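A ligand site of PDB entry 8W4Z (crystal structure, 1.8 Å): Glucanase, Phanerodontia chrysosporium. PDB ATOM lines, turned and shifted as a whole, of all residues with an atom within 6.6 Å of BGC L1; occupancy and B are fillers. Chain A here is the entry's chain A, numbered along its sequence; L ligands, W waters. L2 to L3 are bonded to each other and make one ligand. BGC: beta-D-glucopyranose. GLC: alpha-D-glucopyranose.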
ATOM      1  N   TRP A  48     -17.642 -10.364  16.266  1.00  0.00           N
ATOM      2  CA  TRP A  48     -17.544  -9.052  16.872  1.00  0.00           C
ATOM      3  C   TRP A  48     -18.900  -8.586  17.395  1.00  0.00           C
ATOM      4  O   TRP A  48     -19.906  -8.615  16.673  1.00  0.00           O
ATOM      5  CB  TRP A  48     -16.995  -8.035  15.880  1.00  0.00           C
ATOM      6  CG  TRP A  48     -15.599  -8.246  15.497  1.00  0.00           C
ATOM      7  CD1 TRP A  48     -15.063  -9.375  14.954  1.00  0.00           C
ATOM      8  CD2 TRP A  48     -14.531  -7.293  15.576  1.00  0.00           C
ATOM      9  NE1 TRP A  48     -13.700  -9.201  14.713  1.00  0.00           N
ATOM     10  CE2 TRP A  48     -13.371  -7.915  15.063  1.00  0.00           C
ATOM     11  CE3 TRP A  48     -14.448  -5.991  16.036  1.00  0.00           C
ATOM     12  CZ2 TRP A  48     -12.149  -7.241  15.016  1.00  0.00           C
ATOM     13  CZ3 TRP A  48     -13.254  -5.336  15.952  1.00  0.00           C
ATOM     14  CH2 TRP A  48     -12.114  -5.963  15.471  1.00  0.00           C
ATOM     15  N   LEU A  49     -18.926  -8.180  18.670  1.00  0.00           N
ATOM     16  CA  LEU A  49     -20.121  -7.556  19.248  1.00  0.00           C
ATOM     17  C   LEU A  49     -19.916  -6.046  19.135  1.00  0.00           C
ATOM     18  O   LEU A  49     -19.556  -5.359  20.085  1.00  0.00           O
ATOM     19  CB  LEU A  49     -20.331  -7.985  20.688  1.00  0.00           C
ATOM     20  CG  LEU A  49     -20.442  -9.492  20.919  1.00  0.00           C
ATOM     21  CD1 LEU A  49     -20.664  -9.811  22.394  1.00  0.00           C
ATOM     22  CD2 LEU A  49     -21.589 -10.090  20.101  1.00  0.00           C
ATOM     23  N   ASP A  50     -20.117  -5.533  17.896  1.00  0.00           N
ATOM     24  CA  ASP A  50     -19.853  -4.137  17.578  1.00  0.00           C
ATOM     25  C   ASP A  50     -21.063  -3.251  17.754  1.00  0.00           C
ATOM     26  O   ASP A  50     -20.986  -2.046  17.444  1.00  0.00           O
ATOM     27  CB  ASP A  50     -19.318  -4.009  16.137  1.00  0.00           C
ATOM     28  CG  ASP A  50     -20.281  -4.527  15.127  1.00  0.00           C
ATOM     29  OD1 ASP A  50     -20.995  -5.535  15.361  1.00  0.00           O
ATOM     30  OD2 ASP A  50     -20.379  -3.913  14.043  1.00  0.00           O
ATOM     31  N   LYS A  54     -26.395  -6.843  18.697  1.00  0.00           N
ATOM     32  CA  LYS A  54     -25.898  -8.184  18.452  1.00  0.00           C
ATOM     33  C   LYS A  54     -25.855  -9.047  19.702  1.00  0.00           C
ATOM     34  O   LYS A  54     -25.502 -10.222  19.604  1.00  0.00           O
ATOM     35  CB  LYS A  54     -24.527  -8.115  17.827  1.00  0.00           C
ATOM     36  CG  LYS A  54     -24.605  -7.521  16.413  1.00  0.00           C
ATOM     37  CD  LYS A  54     -23.373  -7.798  15.660  1.00  0.00           C
ATOM     38  CE  LYS A  54     -23.517  -7.332  14.213  1.00  0.00           C
ATOM     39  NZ  LYS A  54     -22.197  -7.474  13.528  1.00  0.00           N
ATOM     40  N   TYR A  83     -16.366  -4.638  21.266  1.00  0.00           N
ATOM     41  CA  TYR A  83     -15.958  -3.459  20.475  1.00  0.00           C
ATOM     42  C   TYR A  83     -17.121  -2.482  20.381  1.00  0.00           C
ATOM     43  O   TYR A  83     -17.763  -2.355  19.332  1.00  0.00           O
ATOM     44  CB  TYR A  83     -15.504  -3.912  19.090  1.00  0.00           C
ATOM     45  CG  TYR A  83     -14.902  -2.842  18.180  1.00  0.00           C
ATOM     46  CD1 TYR A  83     -13.772  -2.162  18.537  1.00  0.00           C
ATOM     47  CD2 TYR A  83     -15.492  -2.545  16.966  1.00  0.00           C
ATOM     48  CE1 TYR A  83     -13.238  -1.222  17.717  1.00  0.00           C
ATOM     49  CE2 TYR A  83     -14.939  -1.609  16.119  1.00  0.00           C
ATOM     50  CZ  TYR A  83     -13.818  -0.943  16.491  1.00  0.00           C
ATOM     51  OH  TYR A  83     -13.240  -0.008  15.666  1.00  0.00           O
ATOM     52  N   ARG A  88     -15.779   5.498  20.058  1.00  0.00           N
ATOM     53  CA  ARG A  88     -14.937   4.445  19.516  1.00  0.00           C
ATOM     54  C   ARG A  88     -14.047   4.976  18.374  1.00  0.00           C
ATOM     55  O   ARG A  88     -14.396   5.941  17.683  1.00  0.00           O
ATOM     56  CB  ARG A  88     -15.840   3.313  18.997  1.00  0.00           C
ATOM     57  CG  ARG A  88     -15.198   1.948  18.870  1.00  0.00           C
ATOM     58  CD  ARG A  88     -16.280   0.918  18.543  1.00  0.00           C
ATOM     59  NE  ARG A  88     -16.795   1.113  17.188  1.00  0.00           N
ATOM     60  CZ  ARG A  88     -17.857   0.478  16.689  1.00  0.00           C
ATOM     61  NH1 ARG A  88     -18.489  -0.459  17.379  1.00  0.00           N
ATOM     62  NH2 ARG A  88     -18.297   0.790  15.475  1.00  0.00           N
ATOM     63  N   ALA A  94     -13.530   5.810  10.316  1.00  0.00           N
ATOM     64  CA  ALA A  94     -14.289   4.791   9.577  1.00  0.00           C
ATOM     65  C   ALA A  94     -15.160   3.925  10.480  1.00  0.00           C
ATOM     66  O   ALA A  94     -16.185   3.424  10.022  1.00  0.00           O
ATOM     67  CB  ALA A  94     -13.342   3.884   8.788  1.00  0.00           C
ATOM     68  N   SER A  95     -14.753   3.693  11.733  1.00  0.00           N
ATOM     69  CA  SER A  95     -15.465   2.771  12.612  1.00  0.00           C
ATOM     70  C   SER A  95     -16.052   3.475  13.838  1.00  0.00           C
ATOM     71  O   SER A  95     -16.214   2.866  14.886  1.00  0.00           O
ATOM     72  CB  SER A  95     -14.570   1.607  13.029  1.00  0.00           C
ATOM     73  OG  SER A  95     -14.379   0.708  11.931  1.00  0.00           O
ATOM     74  N   ASN A  96     -16.412   4.754  13.687  1.00  0.00           N
ATOM     75  CA  ASN A  96     -17.214   5.435  14.681  1.00  0.00           C
ATOM     76  C   ASN A  96     -18.439   4.580  15.024  1.00  0.00           C
ATOM     77  O   ASN A  96     -19.018   3.935  14.151  1.00  0.00           O
ATOM     78  CB  ASN A  96     -17.637   6.801  14.157  1.00  0.00           C
ATOM     79  CG  ASN A  96     -18.436   7.611  15.179  1.00  0.00           C
ATOM     80  OD1 ASN A  96     -18.206   7.498  16.385  1.00  0.00           O
ATOM     81  ND2 ASN A  96     -19.387   8.423  14.696  1.00  0.00           N
ATOM     82  N   ALA A 218      -6.916  -6.902  13.074  1.00  0.00           N
ATOM     83  CA  ALA A 218      -7.330  -6.124  11.905  1.00  0.00           C
ATOM     84  C   ALA A 218      -6.153  -5.555  11.134  1.00  0.00           C
ATOM     85  O   ALA A 218      -6.327  -4.693  10.267  1.00  0.00           O
ATOM     86  CB  ALA A 218      -8.292  -5.005  12.302  1.00  0.00           C
ATOM     87  N   VAL A 306      -8.914 -12.858  14.028  1.00  0.00           N
ATOM     88  CA  VAL A 306      -9.822 -12.018  14.821  1.00  0.00           C
ATOM     89  C   VAL A 306     -10.674 -11.208  13.859  1.00  0.00           C
ATOM     90  O   VAL A 306     -11.902 -11.342  13.870  1.00  0.00           O
ATOM     91  CB  VAL A 306      -9.065 -11.127  15.828  1.00  0.00           C
ATOM     92  CG1 VAL A 306     -10.025 -10.424  16.743  1.00  0.00           C
ATOM     93  CG2 VAL A 306      -8.108 -12.004  16.636  1.00  0.00           C
ATOM     94  N   LYS A 307     -10.043 -10.339  13.042  1.00  0.00           N
ATOM     95  CA  LYS A 307     -10.753  -9.595  11.991  1.00  0.00           C
ATOM     96  C   LYS A 307     -11.196 -10.566  10.908  1.00  0.00           C
ATOM     97  O   LYS A 307     -10.353 -11.288  10.348  1.00  0.00           O
ATOM     98  CB  LYS A 307      -9.836  -8.521  11.436  1.00  0.00           C
ATOM     99  CG  LYS A 307     -10.322  -7.892  10.152  1.00  0.00           C
ATOM    100  CD  LYS A 307     -11.482  -6.896  10.410  1.00  0.00           C
ATOM    101  CE  LYS A 307     -11.990  -6.341   9.113  1.00  0.00           C
ATOM    102  NZ  LYS A 307     -12.949  -5.229   9.309  1.00  0.00           N
ATOM    103  N   PRO A 308     -12.491 -10.652  10.582  1.00  0.00           N
ATOM    104  CA  PRO A 308     -12.914 -11.644   9.589  1.00  0.00           C
ATOM    105  C   PRO A 308     -12.706 -11.114   8.167  1.00  0.00           C
ATOM    106  O   PRO A 308     -13.308 -10.122   7.776  1.00  0.00           O
ATOM    107  CB  PRO A 308     -14.397 -11.863   9.903  1.00  0.00           C
ATOM    108  CG  PRO A 308     -14.673 -11.123  11.226  1.00  0.00           C
ATOM    109  CD  PRO A 308     -13.640 -10.023  11.257  1.00  0.00           C
ATOM    110  N   GLU A 311     -15.022  -8.650   5.636  1.00  0.00           N
ATOM    111  CA  GLU A 311     -15.696  -7.537   6.264  1.00  0.00           C
ATOM    112  C   GLU A 311     -14.836  -6.289   6.151  1.00  0.00           C
ATOM    113  O   GLU A 311     -13.663  -6.301   6.537  1.00  0.00           O
ATOM    114  CB  GLU A 311     -15.984  -7.907   7.720  1.00  0.00           C
ATOM    115  CG  GLU A 311     -16.936  -9.132   7.825  1.00  0.00           C
ATOM    116  CD  GLU A 311     -17.355  -9.453   9.234  1.00  0.00           C
ATOM    117  OE1 GLU A 311     -16.975  -8.711  10.182  1.00  0.00           O
ATOM    118  OE2 GLU A 311     -18.055 -10.477   9.398  1.00  0.00           O
ATOM    119  N   CYS A 312     -15.439  -5.204   5.659  1.00  0.00           N
ATOM    120  CA  CYS A 312     -14.707  -4.031   5.247  1.00  0.00           C
ATOM    121  C   CYS A 312     -14.139  -3.274   6.450  1.00  0.00           C
ATOM    122  O   CYS A 312     -14.672  -3.332   7.557  1.00  0.00           O
ATOM    123  CB  CYS A 312     -15.628  -3.105   4.428  1.00  0.00           C
ATOM    124  SG  CYS A 312     -14.727  -1.863   3.529  1.00  0.00           S
ATOM    125  N   ASP A 313     -13.025  -2.578   6.204  1.00  0.00           N
ATOM    126  CA  ASP A 313     -12.428  -1.735   7.234  1.00  0.00           C
ATOM    127  C   ASP A 313     -12.948  -0.298   7.233  1.00  0.00           C
ATOM    128  O   ASP A 313     -12.662   0.459   8.178  1.00  0.00           O
ATOM    129  CB  ASP A 313     -10.898  -1.645   7.085  1.00  0.00           C
ATOM    130  CG  ASP A 313     -10.208  -2.970   7.226  1.00  0.00           C
ATOM    131  OD1 ASP A 313     -10.586  -3.730   8.121  1.00  0.00           O
ATOM    132  OD2 ASP A 313      -9.280  -3.219   6.432  1.00  0.00           O
ATOM    133  N   GLY A 314     -13.647   0.105   6.184  1.00  0.00           N
ATOM    134  CA  GLY A 314     -14.087   1.476   6.047  1.00  0.00           C
ATOM    135  C   GLY A 314     -14.341   1.844   4.596  1.00  0.00           C
ATOM    136  O   GLY A 314     -13.781   1.258   3.669  1.00  0.00           O
ATOM    137  N   ARG A 322     -18.547   8.647   7.711  1.00  0.00           N
ATOM    138  CA  ARG A 322     -17.450   7.830   8.221  1.00  0.00           C
ATOM    139  C   ARG A 322     -16.301   7.710   7.223  1.00  0.00           C
ATOM    140  O   ARG A 322     -15.522   6.758   7.285  1.00  0.00           O
ATOM    141  CB  ARG A 322     -17.993   6.460   8.602  1.00  0.00           C
ATOM    142  CG  ARG A 322     -19.074   6.558   9.668  1.00  0.00           C
ATOM    143  CD  ARG A 322     -19.081   5.339  10.593  1.00  0.00           C
ATOM    144  NE  ARG A 322     -19.336   4.127   9.840  1.00  0.00           N
ATOM    145  CZ  ARG A 322     -19.345   2.908  10.362  1.00  0.00           C
ATOM    146  NH1 ARG A 322     -19.090   2.711  11.645  1.00  0.00           N
ATOM    147  NH2 ARG A 322     -19.612   1.875   9.582  1.00  0.00           N
ATOM    148  N   ALA A 339     -17.512   0.335   6.846  1.00  0.00           N
ATOM    149  CA  ALA A 339     -16.855  -0.580   7.766  1.00  0.00           C
ATOM    150  C   ALA A 339     -17.847  -1.611   8.289  1.00  0.00           C
ATOM    151  O   ALA A 339     -18.976  -1.282   8.642  1.00  0.00           O
ATOM    152  CB  ALA A 339     -16.244   0.206   8.922  1.00  0.00           C
ATOM    153  N   GLY A 340     -17.401  -2.867   8.364  1.00  0.00           N
ATOM    154  CA  GLY A 340     -18.222  -3.929   8.910  1.00  0.00           C
ATOM    155  C   GLY A 340     -19.105  -4.640   7.908  1.00  0.00           C
ATOM    156  O   GLY A 340     -19.594  -5.745   8.196  1.00  0.00           O
ATOM    157  N   THR A 341     -19.329  -4.066   6.737  1.00  0.00           N
ATOM    158  CA  THR A 341     -20.189  -4.711   5.753  1.00  0.00           C
ATOM    159  C   THR A 341     -19.356  -5.541   4.781  1.00  0.00           C
ATOM    160  O   THR A 341     -18.130  -5.407   4.705  1.00  0.00           O
ATOM    161  CB  THR A 341     -21.014  -3.654   4.998  1.00  0.00           C
ATOM    162  OG1 THR A 341     -20.156  -2.882   4.151  1.00  0.00           O
ATOM    163  CG2 THR A 341     -21.730  -2.738   5.972  1.00  0.00           C
HETATM  164  C2  BGC L   1     -15.944  -2.618  12.065  1.00  0.00           C
HETATM  165  C3  BGC L   1     -16.882  -3.504  12.800  1.00  0.00           C
HETATM  166  C4  BGC L   1     -16.679  -4.921  12.491  1.00  0.00           C
HETATM  167  C5  BGC L   1     -15.279  -5.342  12.668  1.00  0.00           C
HETATM  168  C6  BGC L   1     -15.036  -6.742  12.185  1.00  0.00           C
HETATM  169  C1  BGC L   1     -14.447  -3.010  12.222  1.00  0.00           C
HETATM  170  O1  BGC L   1     -13.710  -2.309  11.422  1.00  0.00           O
HETATM  171  O2  BGC L   1     -16.099  -1.262  12.476  1.00  0.00           O
HETATM  172  O3  BGC L   1     -18.238  -3.078  12.424  1.00  0.00           O
HETATM  173  O4  BGC L   1     -17.517  -5.647  13.447  1.00  0.00           O
HETATM  174  O5  BGC L   1     -14.363  -4.497  11.877  1.00  0.00           O
HETATM  175  O6  BGC L   1     -15.142  -6.861  10.773  1.00  0.00           O
HETATM  176  C1  GLC L   2      -0.221   3.632  13.215  1.00  0.00           C
HETATM  177  C2  GLC L   2      -0.651   2.184  13.063  1.00  0.00           C
HETATM  178  C3  GLC L   2      -2.083   2.102  12.582  1.00  0.00           C
HETATM  179  C4  GLC L   2      -2.987   2.876  13.486  1.00  0.00           C
HETATM  180  C5  GLC L   2      -2.456   4.355  13.708  1.00  0.00           C
HETATM  181  C6  GLC L   2      -3.411   4.825  14.695  1.00  0.00           C
HETATM  182  O1  GLC L   2      -0.297   4.227  11.908  1.00  0.00           O
HETATM  183  O2  GLC L   2       0.169   1.516  12.115  1.00  0.00           O
HETATM  184  O3  GLC L   2      -2.433   0.683  12.638  1.00  0.00           O
HETATM  185  O4  GLC L   2      -4.331   3.004  12.940  1.00  0.00           O
HETATM  186  O5  GLC L   2      -1.118   4.309  14.109  1.00  0.00           O
HETATM  187  O6  GLC L   2      -3.164   6.337  14.697  1.00  0.00           O
HETATM  188  C2  BGC L   3      -6.691   2.671  13.043  1.00  0.00           C
HETATM  189  C3  BGC L   3      -7.777   1.739  13.467  1.00  0.00           C
HETATM  190  C4  BGC L   3      -7.497   0.339  12.902  1.00  0.00           C
HETATM  191  C5  BGC L   3      -6.141  -0.079  13.314  1.00  0.00           C
HETATM  192  C6  BGC L   3      -5.780  -1.416  12.683  1.00  0.00           C
HETATM  193  C1  BGC L   3      -5.324   2.134  13.466  1.00  0.00           C
HETATM  194  O2  BGC L   3      -6.852   4.005  13.645  1.00  0.00           O
HETATM  195  O3  BGC L   3      -9.054   2.165  12.911  1.00  0.00           O
HETATM  196  O4  BGC L   3      -8.454  -0.559  13.401  1.00  0.00           O
HETATM  197  O5  BGC L   3      -5.140   0.882  12.872  1.00  0.00           O
HETATM  198  O6  BGC L   3      -4.431  -1.804  13.085  1.00  0.00           O
HETATM  199  O   HOH W   1     -18.547  -7.990  12.293  1.00  0.00           O
HETATM  200  O   HOH W   2     -18.670  -0.014  12.096  1.00  0.00           O
HETATM  201  O   HOH W   3     -11.910  -1.135  13.455  1.00  0.00           O
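O6 of BGC L1 lies within hydrogen-bond range of OE1 of Glu 311 (2.7 Å). The side-chain hydroxyl (OG) of Ser 95 lies within hydrogen-bond range of an oxygen (O2) of BGC L1 (2.7 Å). The side-chain carboxylate (OD2) of Asp 50 lies within hydrogen-bond range of an oxygen (O3) of BGC L1, 2.8 Å away. An oxygen (O5) of BGC L1 lies within hydrogen-bond range of the side-chain amino group (NZ) of Lys 307, 3.0 Å away.
The backbone carbonyl oxygen (O) of Asp 50 lies within hydrogen-bond range of the guanidinium group (NH1) of Arg 88. The side-chain amino group (NZ) of Lys 54 lies within salt-bridge range of the side-chain carboxylate (OD1) of Asp 50, 2.9 Å away. The side-chain carboxylate of Asp 313 lies within salt-bridge range of the side-chain amino group of Lys 307. The indole nitrogen (NE1) of Trp 48 is in hydrogen-bond range of the backbone carbonyl oxygen (O) of Val 306. O of Cys 312 lies within hydrogen-bond range of N of Gly 340. The backbone carbonyl oxygen (O) of Tyr 83 lies within hydrogen-bond range of the guanidinium group (NH1) of Arg 88 (2.8 Å). The backbone carbonyl oxygen (O) of Leu 49 is in hydrogen-bond range of the backbone NH (N) of Tyr 83. NH2 of Arg 322 lies within hydrogen-bond range of O of Ala 339 (3.4 Å).
Residues that only touch BGC L1: Trp 48, Pro 308, Gly 340, Tyr 83 and Ala 339. Nine residues have an atom within 4 Å of BGC L1: Trp 48, Asp 50, Tyr 83, Ser 95, Lys 307, Pro 308, Glu 311, Ala 339 and Gly 340.
Water W1 bridges OE1 of Glu 311 and O4 of BGC L1. Water W2 lies within hydrogen-bond range of the guanidinium group (NH1) of Arg 322 (2.8 Å), an oxygen (O2) of BGC L1 (2.9 Å) and the guanidinium group (NH2) of Arg 88 (3.5 Å). Water W3 lies within hydrogen-bond range of the side-chain hydroxyl of Tyr 83 (2.8 Å), an oxygen (O1) of BGC L1 (3.0 Å) and the side-chain hydroxyl of Ser 95 (3.4 Å).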
